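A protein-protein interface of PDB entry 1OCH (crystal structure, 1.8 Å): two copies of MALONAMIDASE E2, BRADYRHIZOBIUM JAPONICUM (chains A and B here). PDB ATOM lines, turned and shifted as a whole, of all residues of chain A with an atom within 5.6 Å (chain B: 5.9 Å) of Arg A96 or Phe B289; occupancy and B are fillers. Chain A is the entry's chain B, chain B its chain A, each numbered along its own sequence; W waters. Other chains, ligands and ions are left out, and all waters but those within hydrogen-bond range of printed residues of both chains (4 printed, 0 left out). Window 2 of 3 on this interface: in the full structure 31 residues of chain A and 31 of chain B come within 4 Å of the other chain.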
ATOM      1  N   GLN A  49      20.306 -19.123  10.322  1.00  0.00           N
ATOM      2  CA  GLN A  49      19.468 -19.238  11.507  1.00  0.00           C
ATOM      3  C   GLN A  49      19.484 -20.727  11.854  1.00  0.00           C
ATOM      4  O   GLN A  49      19.785 -21.560  10.999  1.00  0.00           O
ATOM      5  CB  GLN A  49      18.039 -18.758  11.229  1.00  0.00           C
ATOM      6  CG  GLN A  49      17.933 -17.268  10.885  1.00  0.00           C
ATOM      7  CD  GLN A  49      16.522 -16.729  11.063  1.00  0.00           C
ATOM      8  OE1 GLN A  49      15.990 -16.720  12.173  1.00  0.00           O
ATOM      9  NE2 GLN A  49      15.907 -16.284   9.969  1.00  0.00           N
ATOM     10  N   GLY A  52      13.750 -23.531  11.155  1.00  0.00           N
ATOM     11  CA  GLY A  52      12.877 -23.084  10.090  1.00  0.00           C
ATOM     12  C   GLY A  52      13.156 -23.787   8.778  1.00  0.00           C
ATOM     13  O   GLY A  52      14.278 -24.230   8.545  1.00  0.00           O
ATOM     14  N   VAL A  91      10.007  -9.566   3.560  1.00  0.00           N
ATOM     15  CA  VAL A  91      11.327  -9.878   4.082  1.00  0.00           C
ATOM     16  C   VAL A  91      11.129 -10.635   5.397  1.00  0.00           C
ATOM     17  O   VAL A  91      11.818 -11.616   5.674  1.00  0.00           O
ATOM     18  CB  VAL A  91      12.147  -8.601   4.351  1.00  0.00           C
ATOM     19  CG1 VAL A  91      13.420  -8.952   5.111  1.00  0.00           C
ATOM     20  CG2 VAL A  91      12.484  -7.916   3.028  1.00  0.00           C
ATOM     21  N   MET A  92      10.180 -10.174   6.205  1.00  0.00           N
ATOM     22  CA  MET A  92       9.889 -10.832   7.466  1.00  0.00           C
ATOM     23  C   MET A  92       9.359 -12.251   7.227  1.00  0.00           C
ATOM     24  O   MET A  92       9.586 -13.139   8.044  1.00  0.00           O
ATOM     25  CB  MET A  92       8.871 -10.025   8.280  1.00  0.00           C
ATOM     26  CG  MET A  92       9.435  -8.758   8.925  1.00  0.00           C
ATOM     27  SD  MET A  92      10.873  -9.079   9.992  1.00  0.00           S
ATOM     28  CE  MET A  92      10.189 -10.234  11.171  1.00  0.00           C
ATOM     29  N   MET A  93       8.644 -12.459   6.121  1.00  0.00           N
ATOM     30  CA  MET A  93       8.130 -13.797   5.806  1.00  0.00           C
ATOM     31  C   MET A  93       9.321 -14.743   5.643  1.00  0.00           C
ATOM     32  O   MET A  93       9.295 -15.885   6.101  1.00  0.00           O
ATOM     33  CB  MET A  93       7.319 -13.788   4.504  1.00  0.00           C
ATOM     34  CG  MET A  93       5.985 -13.058   4.579  1.00  0.00           C
ATOM     35  SD  MET A  93       5.134 -13.089   2.970  1.00  0.00           S
ATOM     36  CE  MET A  93       3.432 -12.829   3.473  1.00  0.00           C
ATOM     37  N   LEU A  94      10.368 -14.251   4.993  1.00  0.00           N
ATOM     38  CA  LEU A  94      11.563 -15.044   4.781  1.00  0.00           C
ATOM     39  C   LEU A  94      12.288 -15.284   6.109  1.00  0.00           C
ATOM     40  O   LEU A  94      12.629 -16.420   6.446  1.00  0.00           O
ATOM     41  CB  LEU A  94      12.486 -14.332   3.781  1.00  0.00           C
ATOM     42  CG  LEU A  94      11.968 -14.267   2.334  1.00  0.00           C
ATOM     43  CD1 LEU A  94      12.773 -13.261   1.517  1.00  0.00           C
ATOM     44  CD2 LEU A  94      12.047 -15.653   1.703  1.00  0.00           C
ATOM     45  N   LYS A  95      12.503 -14.213   6.869  1.00  0.00           N
ATOM     46  CA  LYS A  95      13.191 -14.317   8.144  1.00  0.00           C
ATOM     47  C   LYS A  95      12.468 -15.242   9.124  1.00  0.00           C
ATOM     48  O   LYS A  95      13.101 -16.035   9.818  1.00  0.00           O
ATOM     49  CB  LYS A  95      13.361 -12.932   8.776  1.00  0.00           C
ATOM     50  CG  LYS A  95      14.027 -11.910   7.869  1.00  0.00           C
ATOM     51  CD  LYS A  95      14.790 -10.847   8.660  1.00  0.00           C
ATOM     52  CE  LYS A  95      14.008 -10.315   9.853  1.00  0.00           C
ATOM     53  NZ  LYS A  95      14.779  -9.273  10.602  1.00  0.00           N
ATOM     54  N   ARG A  96      11.144 -15.143   9.185  1.00  0.00           N
ATOM     55  CA  ARG A  96      10.387 -15.982  10.096  1.00  0.00           C
ATOM     56  C   ARG A  96      10.495 -17.456   9.732  1.00  0.00           C
ATOM     57  O   ARG A  96      10.323 -18.326  10.584  1.00  0.00           O
ATOM     58  CB  ARG A  96       8.920 -15.548  10.128  1.00  0.00           C
ATOM     59  CG  ARG A  96       8.681 -14.288  10.959  1.00  0.00           C
ATOM     60  CD  ARG A  96       7.229 -13.859  10.902  1.00  0.00           C
ATOM     61  NE  ARG A  96       6.925 -12.804  11.864  1.00  0.00           N
ATOM     62  CZ  ARG A  96       5.693 -12.459  12.221  1.00  0.00           C
ATOM     63  NH1 ARG A  96       4.646 -13.083  11.694  1.00  0.00           N
ATOM     64  NH2 ARG A  96       5.502 -11.502  13.118  1.00  0.00           N
ATOM     65  N   ALA A  97      10.795 -17.735   8.468  1.00  0.00           N
ATOM     66  CA  ALA A  97      10.933 -19.104   8.011  1.00  0.00           C
ATOM     67  C   ALA A  97      12.345 -19.643   8.267  1.00  0.00           C
ATOM     68  O   ALA A  97      12.623 -20.816   8.011  1.00  0.00           O
ATOM     69  CB  ALA A  97      10.591 -19.195   6.527  1.00  0.00           C
ATOM     70  N   GLY A  98      13.228 -18.779   8.764  1.00  0.00           N
ATOM     71  CA  GLY A  98      14.594 -19.184   9.062  1.00  0.00           C
ATOM     72  C   GLY A  98      15.636 -18.814   8.018  1.00  0.00           C
ATOM     73  O   GLY A  98      16.795 -19.222   8.117  1.00  0.00           O
ATOM     74  N   ALA A  99      15.238 -18.032   7.021  1.00  0.00           N
ATOM     75  CA  ALA A  99      16.155 -17.627   5.959  1.00  0.00           C
ATOM     76  C   ALA A  99      17.134 -16.533   6.370  1.00  0.00           C
ATOM     77  O   ALA A  99      16.952 -15.854   7.384  1.00  0.00           O
ATOM     78  CB  ALA A  99      15.365 -17.167   4.738  1.00  0.00           C
ATOM     79  N   HIS B 282      -0.950  -9.254  11.036  1.00  0.00           N
ATOM     80  CA  HIS B 282       0.207 -10.021  11.467  1.00  0.00           C
ATOM     81  C   HIS B 282       1.324  -9.959  10.434  1.00  0.00           C
ATOM     82  O   HIS B 282       2.504  -9.959  10.788  1.00  0.00           O
ATOM     83  CB  HIS B 282      -0.188 -11.467  11.754  1.00  0.00           C
ATOM     84  CG  HIS B 282      -0.560 -11.701  13.183  1.00  0.00           C
ATOM     85  ND1 HIS B 282       0.363 -11.639  14.204  1.00  0.00           N
ATOM     86  CD2 HIS B 282      -1.756 -11.937  13.769  1.00  0.00           C
ATOM     87  CE1 HIS B 282      -0.249 -11.826  15.359  1.00  0.00           C
ATOM     88  NE2 HIS B 282      -1.535 -12.009  15.124  1.00  0.00           N
ATOM     89  N   ARG B 283       0.951  -9.895   9.157  1.00  0.00           N
ATOM     90  CA  ARG B 283       1.935  -9.796   8.081  1.00  0.00           C
ATOM     91  C   ARG B 283       2.451  -8.367   7.998  1.00  0.00           C
ATOM     92  O   ARG B 283       3.656  -8.137   7.932  1.00  0.00           O
ATOM     93  CB  ARG B 283       1.314 -10.145   6.721  1.00  0.00           C
ATOM     94  CG  ARG B 283       1.308 -11.622   6.328  1.00  0.00           C
ATOM     95  CD  ARG B 283       0.359 -12.444   7.171  1.00  0.00           C
ATOM     96  NE  ARG B 283       1.063 -13.149   8.233  1.00  0.00           N
ATOM     97  CZ  ARG B 283       0.466 -13.831   9.204  1.00  0.00           C
ATOM     98  NH1 ARG B 283      -0.856 -13.900   9.256  1.00  0.00           N
ATOM     99  NH2 ARG B 283       1.198 -14.450  10.125  1.00  0.00           N
ATOM    100  N   LEU B 285       2.497  -6.035  10.217  1.00  0.00           N
ATOM    101  CA  LEU B 285       3.251  -5.601  11.389  1.00  0.00           C
ATOM    102  C   LEU B 285       4.210  -6.693  11.866  1.00  0.00           C
ATOM    103  O   LEU B 285       4.561  -6.755  13.047  1.00  0.00           O
ATOM    104  CB  LEU B 285       2.285  -5.227  12.520  1.00  0.00           C
ATOM    105  CG  LEU B 285       1.368  -4.035  12.240  1.00  0.00           C
ATOM    106  CD1 LEU B 285       0.377  -3.861  13.382  1.00  0.00           C
ATOM    107  CD2 LEU B 285       2.208  -2.782  12.052  1.00  0.00           C
ATOM    108  N   ALA B 286       4.644  -7.540  10.939  1.00  0.00           N
ATOM    109  CA  ALA B 286       5.545  -8.642  11.270  1.00  0.00           C
ATOM    110  C   ALA B 286       6.822  -8.194  11.970  1.00  0.00           C
ATOM    111  O   ALA B 286       7.209  -8.759  12.994  1.00  0.00           O
ATOM    112  CB  ALA B 286       5.893  -9.421  10.010  1.00  0.00           C
ATOM    113  N   TRP B 287       7.480  -7.183  11.418  1.00  0.00           N
ATOM    114  CA  TRP B 287       8.711  -6.693  12.001  1.00  0.00           C
ATOM    115  C   TRP B 287       8.496  -6.235  13.440  1.00  0.00           C
ATOM    116  O   TRP B 287       9.244  -6.625  14.339  1.00  0.00           O
ATOM    117  CB  TRP B 287       9.268  -5.540  11.168  1.00  0.00           C
ATOM    118  CG  TRP B 287      10.534  -4.971  11.719  1.00  0.00           C
ATOM    119  CD1 TRP B 287      11.793  -5.483  11.587  1.00  0.00           C
ATOM    120  CD2 TRP B 287      10.666  -3.776  12.495  1.00  0.00           C
ATOM    121  NE1 TRP B 287      12.701  -4.679  12.228  1.00  0.00           N
ATOM    122  CE2 TRP B 287      12.038  -3.624  12.796  1.00  0.00           C
ATOM    123  CE3 TRP B 287       9.759  -2.817  12.963  1.00  0.00           C
ATOM    124  CZ2 TRP B 287      12.526  -2.550  13.544  1.00  0.00           C
ATOM    125  CZ3 TRP B 287      10.246  -1.746  13.709  1.00  0.00           C
ATOM    126  CH2 TRP B 287      11.617  -1.625  13.990  1.00  0.00           C
ATOM    127  N   GLU B 288       7.475  -5.412  13.659  1.00  0.00           N
ATOM    128  CA  GLU B 288       7.176  -4.913  15.000  1.00  0.00           C
ATOM    129  C   GLU B 288       6.853  -6.030  15.995  1.00  0.00           C
ATOM    130  O   GLU B 288       7.356  -6.039  17.125  1.00  0.00           O
ATOM    131  CB  GLU B 288       6.002  -3.922  14.963  1.00  0.00           C
ATOM    132  CG  GLU B 288       6.300  -2.600  14.264  1.00  0.00           C
ATOM    133  CD  GLU B 288       6.113  -2.657  12.754  1.00  0.00           C
ATOM    134  OE1 GLU B 288       6.013  -3.767  12.186  1.00  0.00           O
ATOM    135  OE2 GLU B 288       6.074  -1.578  12.133  1.00  0.00           O
ATOM    136  N   PHE B 289       6.019  -6.971  15.566  1.00  0.00           N
ATOM    137  CA  PHE B 289       5.602  -8.084  16.412  1.00  0.00           C
ATOM    138  C   PHE B 289       6.748  -9.050  16.736  1.00  0.00           C
ATOM    139  O   PHE B 289       6.824  -9.582  17.844  1.00  0.00           O
ATOM    140  CB  PHE B 289       4.458  -8.843  15.727  1.00  0.00           C
ATOM    141  CG  PHE B 289       3.820  -9.899  16.589  1.00  0.00           C
ATOM    142  CD1 PHE B 289       2.852  -9.561  17.526  1.00  0.00           C
ATOM    143  CD2 PHE B 289       4.187 -11.236  16.457  1.00  0.00           C
ATOM    144  CE1 PHE B 289       2.252 -10.536  18.324  1.00  0.00           C
ATOM    145  CE2 PHE B 289       3.595 -12.221  17.249  1.00  0.00           C
ATOM    146  CZ  PHE B 289       2.625 -11.868  18.185  1.00  0.00           C
ATOM    147  N   SER B 290       7.638  -9.268  15.773  1.00  0.00           N
ATOM    148  CA  SER B 290       8.762 -10.179  15.960  1.00  0.00           C
ATOM    149  C   SER B 290       9.970  -9.576  16.680  1.00  0.00           C
ATOM    150  O   SER B 290      10.607 -10.249  17.485  1.00  0.00           O
ATOM    151  CB  SER B 290       9.232 -10.732  14.608  1.00  0.00           C
ATOM    152  OG  SER B 290       8.277 -11.620  14.048  1.00  0.00           O
ATOM    153  N   GLU B 291      10.272  -8.311  16.401  1.00  0.00           N
ATOM    154  CA  GLU B 291      11.448  -7.658  16.978  1.00  0.00           C
ATOM    155  C   GLU B 291      11.199  -6.693  18.139  1.00  0.00           C
ATOM    156  O   GLU B 291      12.120  -6.382  18.902  1.00  0.00           O
ATOM    157  CB  GLU B 291      12.188  -6.883  15.885  1.00  0.00           C
ATOM    158  CG  GLU B 291      12.337  -7.601  14.562  1.00  0.00           C
ATOM    159  CD  GLU B 291      13.426  -8.647  14.573  1.00  0.00           C
ATOM    160  OE1 GLU B 291      13.845  -9.069  13.471  1.00  0.00           O
ATOM    161  OE2 GLU B 291      13.861  -9.051  15.674  1.00  0.00           O
ATOM    162  N   HIS B 292       9.971  -6.206  18.264  1.00  0.00           N
ATOM    163  CA  HIS B 292       9.651  -5.249  19.314  1.00  0.00           C
ATOM    164  C   HIS B 292       8.303  -5.538  19.938  1.00  0.00           C
ATOM    165  O   HIS B 292       7.548  -4.619  20.268  1.00  0.00           O
ATOM    166  CB  HIS B 292       9.667  -3.842  18.717  1.00  0.00           C
ATOM    167  CG  HIS B 292      10.979  -3.477  18.096  1.00  0.00           C
ATOM    168  ND1 HIS B 292      12.031  -2.967  18.826  1.00  0.00           N
ATOM    169  CD2 HIS B 292      11.440  -3.635  16.832  1.00  0.00           C
ATOM    170  CE1 HIS B 292      13.083  -2.829  18.040  1.00  0.00           C
ATOM    171  NE2 HIS B 292      12.752  -3.228  16.825  1.00  0.00           N
ATOM    172  N   HIS B 293       8.020  -6.824  20.109  1.00  0.00           N
ATOM    173  CA  HIS B 293       6.768  -7.294  20.664  1.00  0.00           C
ATOM    174  C   HIS B 293       6.303  -6.561  21.911  1.00  0.00           C
ATOM    175  O   HIS B 293       5.203  -6.010  21.937  1.00  0.00           O
ATOM    176  CB  HIS B 293       6.868  -8.795  20.961  1.00  0.00           C
ATOM    177  CG  HIS B 293       5.589  -9.403  21.447  1.00  0.00           C
ATOM    178  ND1 HIS B 293       5.229  -9.422  22.778  1.00  0.00           N
ATOM    179  CD2 HIS B 293       4.570  -9.990  20.775  1.00  0.00           C
ATOM    180  CE1 HIS B 293       4.045  -9.994  22.905  1.00  0.00           C
ATOM    181  NE2 HIS B 293       3.623 -10.347  21.704  1.00  0.00           N
ATOM    182  N   ILE B 296       4.934  -2.970  21.651  1.00  0.00           N
ATOM    183  CA  ILE B 296       3.662  -2.702  21.002  1.00  0.00           C
ATOM    184  C   ILE B 296       2.656  -2.372  22.101  1.00  0.00           C
ATOM    185  O   ILE B 296       2.581  -3.081  23.111  1.00  0.00           O
ATOM    186  CB  ILE B 296       3.170  -3.933  20.207  1.00  0.00           C
ATOM    187  CG1 ILE B 296       4.144  -4.230  19.066  1.00  0.00           C
ATOM    188  CG2 ILE B 296       1.749  -3.688  19.681  1.00  0.00           C
ATOM    189  CD1 ILE B 296       3.804  -5.478  18.261  1.00  0.00           C
ATOM    190  N   ARG B 301      -1.204  -5.210  21.142  1.00  0.00           N
ATOM    191  CA  ARG B 301      -0.360  -6.359  21.411  1.00  0.00           C
ATOM    192  C   ARG B 301      -1.224  -7.563  21.768  1.00  0.00           C
ATOM    193  O   ARG B 301      -0.940  -8.690  21.357  1.00  0.00           O
ATOM    194  CB  ARG B 301       0.614  -6.056  22.556  1.00  0.00           C
ATOM    195  CG  ARG B 301       1.671  -7.136  22.747  1.00  0.00           C
ATOM    196  CD  ARG B 301       2.777  -6.713  23.709  1.00  0.00           C
ATOM    197  NE  ARG B 301       2.348  -6.704  25.104  1.00  0.00           N
ATOM    198  CZ  ARG B 301       2.331  -5.622  25.875  1.00  0.00           C
ATOM    199  NH1 ARG B 301       2.717  -4.447  25.393  1.00  0.00           N
ATOM    200  NH2 ARG B 301       1.940  -5.717  27.138  1.00  0.00           N
ATOM    201  N   LEU B 304      -3.130  -8.937  18.618  1.00  0.00           N
ATOM    202  CA  LEU B 304      -2.207  -9.664  17.754  1.00  0.00           C
ATOM    203  C   LEU B 304      -1.883 -11.025  18.386  1.00  0.00           C
ATOM    204  O   LEU B 304      -1.865 -12.052  17.714  1.00  0.00           O
ATOM    205  CB  LEU B 304      -0.928  -8.848  17.537  1.00  0.00           C
ATOM    206  CG  LEU B 304      -1.053  -7.611  16.633  1.00  0.00           C
ATOM    207  CD1 LEU B 304       0.129  -6.670  16.840  1.00  0.00           C
ATOM    208  CD2 LEU B 304      -1.135  -8.060  15.181  1.00  0.00           C
ATOM    209  N   ASP B 305      -1.639 -11.025  19.690  1.00  0.00           N
ATOM    210  CA  ASP B 305      -1.330 -12.255  20.403  1.00  0.00           C
ATOM    211  C   ASP B 305      -2.453 -13.286  20.304  1.00  0.00           C
ATOM    212  O   ASP B 305      -2.196 -14.477  20.158  1.00  0.00           O
ATOM    213  CB  ASP B 305      -1.052 -11.953  21.874  1.00  0.00           C
ATOM    214  CG  ASP B 305       0.352 -11.441  22.108  1.00  0.00           C
ATOM    215  OD1 ASP B 305       0.612 -10.905  23.207  1.00  0.00           O
ATOM    216  OD2 ASP B 305       1.202 -11.584  21.203  1.00  0.00           O
ATOM    217  N   VAL B 308      -2.480 -14.937  16.411  1.00  0.00           N
ATOM    218  CA  VAL B 308      -1.328 -15.501  15.711  1.00  0.00           C
ATOM    219  C   VAL B 308      -1.677 -16.803  14.986  1.00  0.00           C
ATOM    220  O   VAL B 308      -1.001 -17.188  14.032  1.00  0.00           O
ATOM    221  CB  VAL B 308      -0.150 -15.803  16.676  1.00  0.00           C
ATOM    222  CG1 VAL B 308       0.295 -14.532  17.370  1.00  0.00           C
ATOM    223  CG2 VAL B 308      -0.557 -16.854  17.684  1.00  0.00           C
HETATM  224  O   HOH W   1       3.064 -10.567  13.422  1.00  0.00           O
HETATM  225  O   HOH W   2       2.472 -13.830  13.648  1.00  0.00           O
HETATM  226  O   HOH W   3       4.046 -15.597  10.166  1.00  0.00           O
HETATM  227  O   HOH W   4       4.291 -13.012   8.381  1.00  0.00           O
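The guanidinium group (NH2) of Arg A96 lies within hydrogen-bond range of the backbone carbonyl oxygen (O) of Ala B286.
The side-chain amino group of Lys A95 is in salt-bridge range of the side-chain carboxylate of Glu B291 (3.0 Å).
The side-chain hydroxyl (OG) of Ser B290 is in hydrogen-bond range of the guanidinium group (NE) of Arg A96 (2.8 Å).
Water W1 bridges NH2 of Arg A96 and O of His B282.
Water W3 bridges NH1 of Arg A96 (3.0 Å) and NH2 of Arg B283 (3.1 Å).
Water W2 bridges the guanidinium group of Arg A96 (3.0 Å) and a ring nitrogen (ND1) of His B282 (3.1 Å).
Water W4 bridges NE of Arg B283 (3.2 Å) and NH1 of Arg A96 (3.3 Å).
Of the 16 printed residues of chain B, 7 touch a printed residue of chain A.
Printed residues of chain A that touch a printed residue of chain B: Met A92, Met A93, Lys A95 and Arg A96.
Hydrophobic or aromatic side chains of chain A within 4 Å of the printed part of chain B: Met A92 and Met A93.
Among the printed residues, 9 pairs touch across the chains.
Among the printed residues, Asp or Glu carboxylates within 4 Å of a Lys or Arg side-chain nitrogen of the other chain: Lys A95 with Glu B291 (3.0 Å).
No position is printed for both chains.
Of the 9 pairs that touch across the chains among the printed residues, none has its exchanged pair printed and touching as well.
Among the printed residues, merely in contact across the chains: Met A92 with Ala B286 (3.5 Å), Met A92 with Trp B287 (3.5 Å), Met A92 with Ser B290 (3.6 Å), Met A93 with Arg B283 (3.8 Å), Arg A96 with His B282 (3.9 Å) and Arg A96 with Phe B289 (3.6 Å).
Of the printed residues of chain B, Met A92 touches Ala B286, Trp B287 and Ser B290.
Of chain B, only His B282 (3.9 Å), Ala B286 (3.2 Å), Phe B289 (3.6 Å) and Ser B290 (2.8 Å) come within 4 Å of Arg A96.
Printed residues of chain A within 4 Å of His B282: Arg A96 (3.9 Å).
Printed residues of chain A within 4 Å of Ala B286: Met A92 (3.5 Å) and Arg A96 (3.2 Å).
Of the printed residues of chain A, Trp B287 touches Met A92.
Printed residues of chain A within 4 Å of Phe B289: Arg A96 (3.6 Å).
Of the printed residues of chain A, Ser B290 touches Met A92 (3.6 Å) and Arg A96 (2.8 Å).
The nearest printed residue of chain A that does not touch Phe B289 is Met A92 (6.6 Å).
The nearest printed residue of chain B that does not touch Met A93 is Ala B286 (5.6 Å).
NE2 of His B282 is in hydrogen-bond range of N of Val B308, at 3.3 Å.
NE2 of His B282 is in hydrogen-bond range of O of Leu B304 (2.6 Å).
O of Lys A95 is in hydrogen-bond range of NE2 of Gln A49 (2.8 Å).
The side-chain hydroxyl of Ser B290 sits at hydrogen-bond distance from the backbone carbonyl oxygen of Ala B286, 3.2 Å away.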
